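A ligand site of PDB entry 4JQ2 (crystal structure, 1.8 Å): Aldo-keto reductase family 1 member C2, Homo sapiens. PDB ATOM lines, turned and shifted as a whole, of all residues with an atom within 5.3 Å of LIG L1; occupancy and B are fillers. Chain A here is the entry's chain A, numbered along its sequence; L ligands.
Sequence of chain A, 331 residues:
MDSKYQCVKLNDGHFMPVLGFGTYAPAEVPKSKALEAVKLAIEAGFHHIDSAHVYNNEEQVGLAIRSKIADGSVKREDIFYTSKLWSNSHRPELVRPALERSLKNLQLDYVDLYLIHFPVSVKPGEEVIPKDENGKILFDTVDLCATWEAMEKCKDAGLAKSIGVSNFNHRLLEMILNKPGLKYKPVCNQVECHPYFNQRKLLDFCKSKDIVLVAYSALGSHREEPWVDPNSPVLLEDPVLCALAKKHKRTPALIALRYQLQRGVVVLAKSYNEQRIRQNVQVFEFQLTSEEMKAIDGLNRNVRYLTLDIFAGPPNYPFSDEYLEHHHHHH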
ATOM      1  N   TYR A  24       6.512  13.311  24.019  1.00  0.00           N
ATOM      2  CA  TYR A  24       6.271  11.876  23.870  1.00  0.00           C
ATOM      3  C   TYR A  24       5.317  11.646  22.725  1.00  0.00           C
ATOM      4  O   TYR A  24       4.256  12.293  22.637  1.00  0.00           O
ATOM      5  CB  TYR A  24       5.654  11.259  25.106  1.00  0.00           C
ATOM      6  CG  TYR A  24       5.241   9.813  24.859  1.00  0.00           C
ATOM      7  CD1 TYR A  24       6.207   8.794  24.845  1.00  0.00           C
ATOM      8  CD2 TYR A  24       3.907   9.492  24.557  1.00  0.00           C
ATOM      9  CE1 TYR A  24       5.833   7.463  24.578  1.00  0.00           C
ATOM     10  CE2 TYR A  24       3.523   8.201  24.274  1.00  0.00           C
ATOM     11  CZ  TYR A  24       4.470   7.187  24.282  1.00  0.00           C
ATOM     12  OH  TYR A  24       4.020   5.912  23.989  1.00  0.00           O
ATOM     13  N   VAL A  54      12.981   7.465  28.870  1.00  0.00           N
ATOM     14  CA  VAL A  54      12.080   6.366  28.406  1.00  0.00           C
ATOM     15  C   VAL A  54      11.355   6.682  27.102  1.00  0.00           C
ATOM     16  O   VAL A  54      10.868   5.757  26.420  1.00  0.00           O
ATOM     17  CB  VAL A  54      11.143   6.001  29.581  1.00  0.00           C
ATOM     18  CG1 VAL A  54       9.884   6.841  29.603  1.00  0.00           C
ATOM     19  CG2 VAL A  54      10.808   4.515  29.601  1.00  0.00           C
ATOM     20  N   TYR A  55      11.298   7.968  26.722  1.00  0.00           N
ATOM     21  CA  TYR A  55      10.681   8.380  25.457  1.00  0.00           C
ATOM     22  C   TYR A  55      11.505   8.022  24.260  1.00  0.00           C
ATOM     23  O   TYR A  55      10.965   8.004  23.144  1.00  0.00           O
ATOM     24  CB  TYR A  55      10.289   9.878  25.362  1.00  0.00           C
ATOM     25  CG  TYR A  55       9.385  10.396  26.475  1.00  0.00           C
ATOM     26  CD1 TYR A  55       8.701   9.550  27.281  1.00  0.00           C
ATOM     27  CD2 TYR A  55       9.271  11.745  26.701  1.00  0.00           C
ATOM     28  CE1 TYR A  55       7.890  10.008  28.304  1.00  0.00           C
ATOM     29  CE2 TYR A  55       8.463  12.247  27.735  1.00  0.00           C
ATOM     30  CZ  TYR A  55       7.782  11.380  28.535  1.00  0.00           C
ATOM     31  OH  TYR A  55       7.026  11.878  29.563  1.00  0.00           O
ATOM     32  N   LYS A  84      13.877  13.012  32.713  1.00  0.00           N
ATOM     33  CA  LYS A  84      13.341  12.190  33.781  1.00  0.00           C
ATOM     34  C   LYS A  84      14.157  10.873  33.848  1.00  0.00           C
ATOM     35  O   LYS A  84      14.552  10.235  32.837  1.00  0.00           O
ATOM     36  CB  LYS A  84      11.823  11.885  33.609  1.00  0.00           C
ATOM     37  CG  LYS A  84      11.018  13.119  33.227  1.00  0.00           C
ATOM     38  CD  LYS A  84       9.521  12.833  33.173  1.00  0.00           C
ATOM     39  CE  LYS A  84       8.734  13.989  32.546  1.00  0.00           C
ATOM     40  NZ  LYS A  84       8.571  13.877  31.074  1.00  0.00           N
ATOM     41  N   TRP A  86      14.532   7.218  34.686  1.00  0.00           N
ATOM     42  CA  TRP A  86      13.641   6.025  34.422  1.00  0.00           C
ATOM     43  C   TRP A  86      13.864   5.017  35.568  1.00  0.00           C
ATOM     44  O   TRP A  86      14.882   5.063  36.244  1.00  0.00           O
ATOM     45  CB  TRP A  86      13.795   5.443  32.987  1.00  0.00           C
ATOM     46  CG  TRP A  86      12.792   4.324  32.856  1.00  0.00           C
ATOM     47  CD1 TRP A  86      13.043   2.975  32.673  1.00  0.00           C
ATOM     48  CD2 TRP A  86      11.392   4.442  33.079  1.00  0.00           C
ATOM     49  NE1 TRP A  86      11.854   2.274  32.759  1.00  0.00           N
ATOM     50  CE2 TRP A  86      10.837   3.153  33.004  1.00  0.00           C
ATOM     51  CE3 TRP A  86      10.556   5.515  33.426  1.00  0.00           C
ATOM     52  CZ2 TRP A  86       9.489   2.919  33.195  1.00  0.00           C
ATOM     53  CZ3 TRP A  86       9.174   5.279  33.585  1.00  0.00           C
ATOM     54  CH2 TRP A  86       8.674   3.999  33.475  1.00  0.00           C
ATOM     55  N   HIS A 117      10.749   9.774  37.437  1.00  0.00           N
ATOM     56  CA  HIS A 117       9.643   9.625  36.443  1.00  0.00           C
ATOM     57  C   HIS A 117       8.428   8.908  37.018  1.00  0.00           C
ATOM     58  O   HIS A 117       7.296   9.334  36.841  1.00  0.00           O
ATOM     59  CB  HIS A 117      10.146   8.936  35.212  1.00  0.00           C
ATOM     60  CG  HIS A 117       9.299   9.141  34.007  1.00  0.00           C
ATOM     61  ND1 HIS A 117       9.808   8.949  32.742  1.00  0.00           N
ATOM     62  CD2 HIS A 117       8.031   9.593  33.849  1.00  0.00           C
ATOM     63  CE1 HIS A 117       8.862   9.213  31.855  1.00  0.00           C
ATOM     64  NE2 HIS A 117       7.784   9.617  32.502  1.00  0.00           N
ATOM     65  N   VAL A 128      14.314  -0.928  29.455  1.00  0.00           N
ATOM     66  CA  VAL A 128      13.477  -0.028  30.244  1.00  0.00           C
ATOM     67  C   VAL A 128      12.267  -0.718  30.909  1.00  0.00           C
ATOM     68  O   VAL A 128      11.854  -0.307  32.026  1.00  0.00           O
ATOM     69  CB  VAL A 128      13.017   1.187  29.431  1.00  0.00           C
ATOM     70  CG1 VAL A 128      14.263   1.920  28.888  1.00  0.00           C
ATOM     71  CG2 VAL A 128      12.092   0.770  28.321  1.00  0.00           C
ATOM     72  N   ILE A 129      11.710  -1.741  30.256  1.00  0.00           N
ATOM     73  CA  ILE A 129      10.737  -2.593  30.933  1.00  0.00           C
ATOM     74  C   ILE A 129      11.277  -4.029  30.987  1.00  0.00           C
ATOM     75  O   ILE A 129      10.975  -4.828  30.148  1.00  0.00           O
ATOM     76  CB  ILE A 129       9.377  -2.643  30.212  1.00  0.00           C
ATOM     77  CG1 ILE A 129       8.821  -1.236  29.870  1.00  0.00           C
ATOM     78  CG2 ILE A 129       8.397  -3.405  31.074  1.00  0.00           C
ATOM     79  CD1 ILE A 129       8.474  -0.426  31.054  1.00  0.00           C
ATOM     80  N   HIS A 222      -2.907  11.531  24.497  1.00  0.00           N
ATOM     81  CA  HIS A 222      -2.754  10.855  23.170  1.00  0.00           C
ATOM     82  C   HIS A 222      -3.836   9.763  22.923  1.00  0.00           C
ATOM     83  O   HIS A 222      -4.103   9.405  21.766  1.00  0.00           O
ATOM     84  CB  HIS A 222      -1.312  10.238  23.048  1.00  0.00           C
ATOM     85  CG  HIS A 222      -0.831   9.569  24.319  1.00  0.00           C
ATOM     86  ND1 HIS A 222      -1.399   8.409  24.812  1.00  0.00           N
ATOM     87  CD2 HIS A 222       0.094   9.930  25.235  1.00  0.00           C
ATOM     88  CE1 HIS A 222      -0.821   8.075  25.954  1.00  0.00           C
ATOM     89  NE2 HIS A 222       0.082   8.997  26.240  1.00  0.00           N
ATOM     90  N   GLU A 224      -3.664   6.586  23.284  1.00  0.00           N
ATOM     91  CA  GLU A 224      -2.967   5.482  22.640  1.00  0.00           C
ATOM     92  C   GLU A 224      -3.273   4.180  23.411  1.00  0.00           C
ATOM     93  O   GLU A 224      -3.099   4.134  24.625  1.00  0.00           O
ATOM     94  CB  GLU A 224      -1.457   5.756  22.693  1.00  0.00           C
ATOM     95  CG  GLU A 224      -0.524   4.839  21.904  1.00  0.00           C
ATOM     96  CD  GLU A 224       0.932   4.935  22.370  1.00  0.00           C
ATOM     97  OE1 GLU A 224       1.313   5.866  23.125  1.00  0.00           O
ATOM     98  OE2 GLU A 224       1.719   4.043  21.962  1.00  0.00           O
ATOM     99  N   TRP A 227      -2.509   1.821  26.600  1.00  0.00           N
ATOM    100  CA  TRP A 227      -2.238   2.623  27.811  1.00  0.00           C
ATOM    101  C   TRP A 227      -3.486   3.409  28.307  1.00  0.00           C
ATOM    102  O   TRP A 227      -3.612   3.709  29.520  1.00  0.00           O
ATOM    103  CB  TRP A 227      -1.049   3.567  27.569  1.00  0.00           C
ATOM    104  CG  TRP A 227       0.084   2.855  26.900  1.00  0.00           C
ATOM    105  CD1 TRP A 227       0.413   2.876  25.570  1.00  0.00           C
ATOM    106  CD2 TRP A 227       1.015   1.972  27.533  1.00  0.00           C
ATOM    107  NE1 TRP A 227       1.503   2.055  25.342  1.00  0.00           N
ATOM    108  CE2 TRP A 227       1.893   1.493  26.527  1.00  0.00           C
ATOM    109  CE3 TRP A 227       1.211   1.548  28.861  1.00  0.00           C
ATOM    110  CZ2 TRP A 227       2.935   0.623  26.806  1.00  0.00           C
ATOM    111  CZ3 TRP A 227       2.254   0.670  29.134  1.00  0.00           C
ATOM    112  CH2 TRP A 227       3.103   0.227  28.113  1.00  0.00           C
ATOM    113  N   LEU A 306      -4.418   7.740  32.441  1.00  0.00           N
ATOM    114  CA  LEU A 306      -3.147   7.087  32.374  1.00  0.00           C
ATOM    115  C   LEU A 306      -2.883   6.409  33.709  1.00  0.00           C
ATOM    116  O   LEU A 306      -2.368   7.001  34.637  1.00  0.00           O
ATOM    117  CB  LEU A 306      -2.052   8.069  32.002  1.00  0.00           C
ATOM    118  CG  LEU A 306      -0.898   7.346  31.318  1.00  0.00           C
ATOM    119  CD1 LEU A 306      -1.200   7.006  29.864  1.00  0.00           C
ATOM    120  CD2 LEU A 306       0.346   8.192  31.406  1.00  0.00           C
ATOM    121  N   LEU A 308      -0.964   3.579  33.975  1.00  0.00           N
ATOM    122  CA  LEU A 308       0.295   2.789  33.942  1.00  0.00           C
ATOM    123  C   LEU A 308       0.189   1.502  34.793  1.00  0.00           C
ATOM    124  O   LEU A 308       1.103   1.189  35.580  1.00  0.00           O
ATOM    125  CB  LEU A 308       1.483   3.620  34.422  1.00  0.00           C
ATOM    126  CG  LEU A 308       1.642   4.952  33.676  1.00  0.00           C
ATOM    127  CD1 LEU A 308       2.771   5.854  34.206  1.00  0.00           C
ATOM    128  CD2 LEU A 308       1.820   4.610  32.212  1.00  0.00           C
ATOM    129  N   ILE A 310       0.523  -1.502  34.320  1.00  0.00           N
ATOM    130  CA  ILE A 310       1.523  -2.551  34.190  1.00  0.00           C
ATOM    131  C   ILE A 310       2.481  -2.517  35.407  1.00  0.00           C
ATOM    132  O   ILE A 310       3.086  -3.541  35.727  1.00  0.00           O
ATOM    133  CB  ILE A 310       2.307  -2.500  32.857  1.00  0.00           C
ATOM    134  CG1 ILE A 310       3.145  -1.231  32.771  1.00  0.00           C
ATOM    135  CG2 ILE A 310       1.356  -2.609  31.667  1.00  0.00           C
ATOM    136  CD1 ILE A 310       4.224  -1.344  31.701  1.00  0.00           C
ATOM    137  N   PHE A 311       2.563  -1.380  36.125  1.00  0.00           N
ATOM    138  CA  PHE A 311       3.375  -1.273  37.350  1.00  0.00           C
ATOM    139  C   PHE A 311       2.590  -1.408  38.626  1.00  0.00           C
ATOM    140  O   PHE A 311       3.110  -1.128  39.715  1.00  0.00           O
ATOM    141  CB  PHE A 311       4.144   0.062  37.393  1.00  0.00           C
ATOM    142  CG  PHE A 311       4.931   0.373  36.159  1.00  0.00           C
ATOM    143  CD1 PHE A 311       5.940  -0.447  35.753  1.00  0.00           C
ATOM    144  CD2 PHE A 311       4.662   1.519  35.384  1.00  0.00           C
ATOM    145  CE1 PHE A 311       6.708  -0.190  34.625  1.00  0.00           C
ATOM    146  CE2 PHE A 311       5.403   1.797  34.228  1.00  0.00           C
ATOM    147  CZ  PHE A 311       6.447   0.914  33.852  1.00  0.00           C
HETATM  148  C1  LIG L   1       6.483   1.013  28.352  1.00  0.00           C
HETATM  149  C2  LIG L   1       6.346   2.070  29.261  1.00  0.00           C
HETATM  150  C3  LIG L   1       6.864   3.326  28.943  1.00  0.00           C
HETATM  151  C4  LIG L   1       6.697   4.378  29.855  1.00  0.00           C
HETATM  152  C5  LIG L   1       5.610   5.173  29.779  1.00  0.00           C
HETATM  153  C6  LIG L   1       4.633   5.274  28.802  1.00  0.00           C
HETATM  154  C7  LIG L   1       4.181   4.397  27.870  1.00  0.00           C
HETATM  155  C8  LIG L   1       3.039   4.698  27.120  1.00  0.00           C
HETATM  156  C9  LIG L   1       2.347   5.864  27.360  1.00  0.00           C
HETATM  157  F1  LIG L   1       1.296   6.149  26.667  1.00  0.00           F
HETATM  158  C10 LIG L   1       2.826   6.761  28.302  1.00  0.00           C
HETATM  159  C11 LIG L   1       3.982   6.467  29.000  1.00  0.00           C
HETATM  160  C12 LIG L   1       4.460   6.952  30.154  1.00  0.00           C
HETATM  161  C13 LIG L   1       4.045   8.301  30.716  1.00  0.00           C
HETATM  162  C14 LIG L   1       4.812   9.462  29.983  1.00  0.00           C
HETATM  163  O1  LIG L   1       5.715  10.055  30.632  1.00  0.00           O
HETATM  164  O2  LIG L   1       4.455   9.794  28.806  1.00  0.00           O
HETATM  165  C15 LIG L   1       5.477   6.211  30.603  1.00  0.00           C
HETATM  166  C16 LIG L   1       6.159   6.372  31.950  1.00  0.00           C
HETATM  167  C17 LIG L   1       7.538   3.537  27.721  1.00  0.00           C
HETATM  168  C18 LIG L   1       7.687   2.475  26.818  1.00  0.00           C
HETATM  169  C19 LIG L   1       7.157   1.223  27.130  1.00  0.00           C
HETATM  170  S1  LIG L   1       7.352  -0.111  25.996  1.00  0.00           S
HETATM  171  O3  LIG L   1       8.865  -0.245  25.756  1.00  0.00           O
HETATM  172  C20 LIG L   1       6.683  -1.685  26.541  1.00  0.00           C
HETATM  173  P1  LG2 L   2      -1.734  15.891  25.797  1.00  0.00           P
HETATM  174  O1  LG2 L   2      -3.070  15.778  26.476  1.00  0.00           O
HETATM  175  O2  LG2 L   2      -1.004  17.166  25.571  1.00  0.00           O
HETATM  176  O3  LG2 L   2      -2.238  15.935  24.188  1.00  0.00           O
HETATM  177  C1  LG2 L   2      -2.938  14.929  23.562  1.00  0.00           C
HETATM  178  C2  LG2 L   2      -3.359  15.215  22.096  1.00  0.00           C
HETATM  179  O4  LG2 L   2      -3.740  16.553  21.835  1.00  0.00           O
HETATM  180  C3  LG2 L   2      -2.161  14.966  21.132  1.00  0.00           C
HETATM  181  O5  LG2 L   2      -2.371  13.710  20.537  1.00  0.00           O
HETATM  182  C4  LG2 L   2      -2.175  16.107  20.069  1.00  0.00           C
HETATM  183  O6  LG2 L   2      -2.204  15.700  18.659  1.00  0.00           O
HETATM  184  C5  LG2 L   2      -3.496  16.827  20.435  1.00  0.00           C
HETATM  185  N1  LG2 L   2      -3.506  18.338  20.396  1.00  0.00           N
HETATM  186  C6  LG2 L   2      -2.511  19.180  20.723  1.00  0.00           C
HETATM  187  N2  LG2 L   2      -2.928  20.439  20.565  1.00  0.00           N
HETATM  188  C7  LG2 L   2      -4.220  20.404  20.107  1.00  0.00           C
HETATM  189  C8  LG2 L   2      -5.102  21.408  19.751  1.00  0.00           C
HETATM  190  N3  LG2 L   2      -4.691  22.687  19.884  1.00  0.00           N
HETATM  191  N4  LG2 L   2      -6.367  21.119  19.297  1.00  0.00           N
HETATM  192  C9  LG2 L   2      -6.717  19.753  19.195  1.00  0.00           C
HETATM  193  N5  LG2 L   2      -5.801  18.727  19.549  1.00  0.00           N
HETATM  194  C10 LG2 L   2      -4.560  19.090  20.006  1.00  0.00           C
HETATM  195  O7  LG2 L   2      -0.924  14.481  25.559  1.00  0.00           O
HETATM  196  P2  LG2 L   2       0.240  13.693  26.518  1.00  0.00           P
HETATM  197  O8  LG2 L   2      -0.768  12.783  27.061  1.00  0.00           O
HETATM  198  O9  LG2 L   2       0.990  13.559  25.211  1.00  0.00           O
HETATM  199  O10 LG2 L   2       0.792  14.721  27.592  1.00  0.00           O
HETATM  200  C11 LG2 L   2       1.616  15.846  27.227  1.00  0.00           C
HETATM  201  C12 LG2 L   2       3.067  15.564  27.561  1.00  0.00           C
HETATM  202  O11 LG2 L   2       3.205  15.352  29.005  1.00  0.00           O
HETATM  203  C13 LG2 L   2       3.745  14.324  26.887  1.00  0.00           C
HETATM  204  O12 LG2 L   2       4.214  14.507  25.522  1.00  0.00           O
HETATM  205  C14 LG2 L   2       4.984  14.195  27.877  1.00  0.00           C
HETATM  206  O13 LG2 L   2       6.031  15.191  27.637  1.00  0.00           O
HETATM  207  C15 LG2 L   2       4.364  14.496  29.251  1.00  0.00           C
HETATM  208  N6  LG2 L   2       3.828  13.306  29.978  1.00  0.00           N
HETATM  209  C16 LG2 L   2       4.483  12.894  31.126  1.00  0.00           C
HETATM  210  C17 LG2 L   2       4.004  11.830  31.852  1.00  0.00           C
HETATM  211  C18 LG2 L   2       4.682  11.416  33.019  1.00  0.00           C
HETATM  212  O14 LG2 L   2       4.529  10.271  33.400  1.00  0.00           O
HETATM  213  N7  LG2 L   2       5.462  12.297  33.691  1.00  0.00           N
HETATM  214  C19 LG2 L   2       2.843  11.143  31.393  1.00  0.00           C
HETATM  215  C20 LG2 L   2       2.174  11.515  30.228  1.00  0.00           C
HETATM  216  C21 LG2 L   2       2.658  12.609  29.514  1.00  0.00           C
HETATM  217  P3  LG2 L   2      -1.200  16.375  17.502  1.00  0.00           P
HETATM  218  O15 LG2 L   2       0.190  15.963  17.902  1.00  0.00           O
HETATM  219  O16 LG2 L   2      -1.568  15.873  16.196  1.00  0.00           O
HETATM  220  O17 LG2 L   2      -1.493  17.815  17.653  1.00  0.00           O
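An oxygen (O14) of LG2 L2 is in hydrogen-bond range of a ring nitrogen (NE2) of His 117, at 3.4 Å.
A ring nitrogen (NE2) of His 117 is in hydrogen-bond range of an oxygen (O1) of LIG L1.
The backbone NH (N) of Tyr 24 is in hydrogen-bond range of an oxygen (O12) of LG2 L2 (3.0 Å).
OH of Tyr 55 lies within hydrogen-bond range of O1 of LIG L1 (2.5 Å).
O1 of LIG L1 sits close to O14 of LG2 L2 (3.0 Å).
The side-chain hydroxyl (OH) of Tyr 24 lies within hydrogen-bond range of the side-chain carboxylate (OE1) of Glu 224.
The backbone carbonyl oxygen of Val 128 lies within hydrogen-bond range of the indole nitrogen of Trp 86 (2.7 Å).
The side-chain amino group (NZ) of Lys 84 sits at hydrogen-bond distance from the side-chain hydroxyl (OH) of Tyr 55, 2.9 Å away.
N of Glu 224 lies close to ND1 of His 222 (3.3 Å).
NE2 of His 222 lies close to F1 of LIG L1 (3.1 Å).
Merely in contact with LIG L1: Trp 227, Tyr 24, Glu 224, Ile 129, Trp 86, Leu 306 and Val 54.
Hydrophobic or aromatic side chains within 4 Å of LIG L1: Tyr 24, Val 54, Tyr 55, Trp 86, His 117, Ile 129, His 222, Trp 227 and Leu 306.
Within 4 Å of LIG L1: Tyr 24, Val 54, Tyr 55, Trp 86, His 117, Ile 129, His 222, Glu 224, Trp 227 and Leu 306.
The nearest printed residue that does not touch LIG L1 is Leu 308 (4.1 Å).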
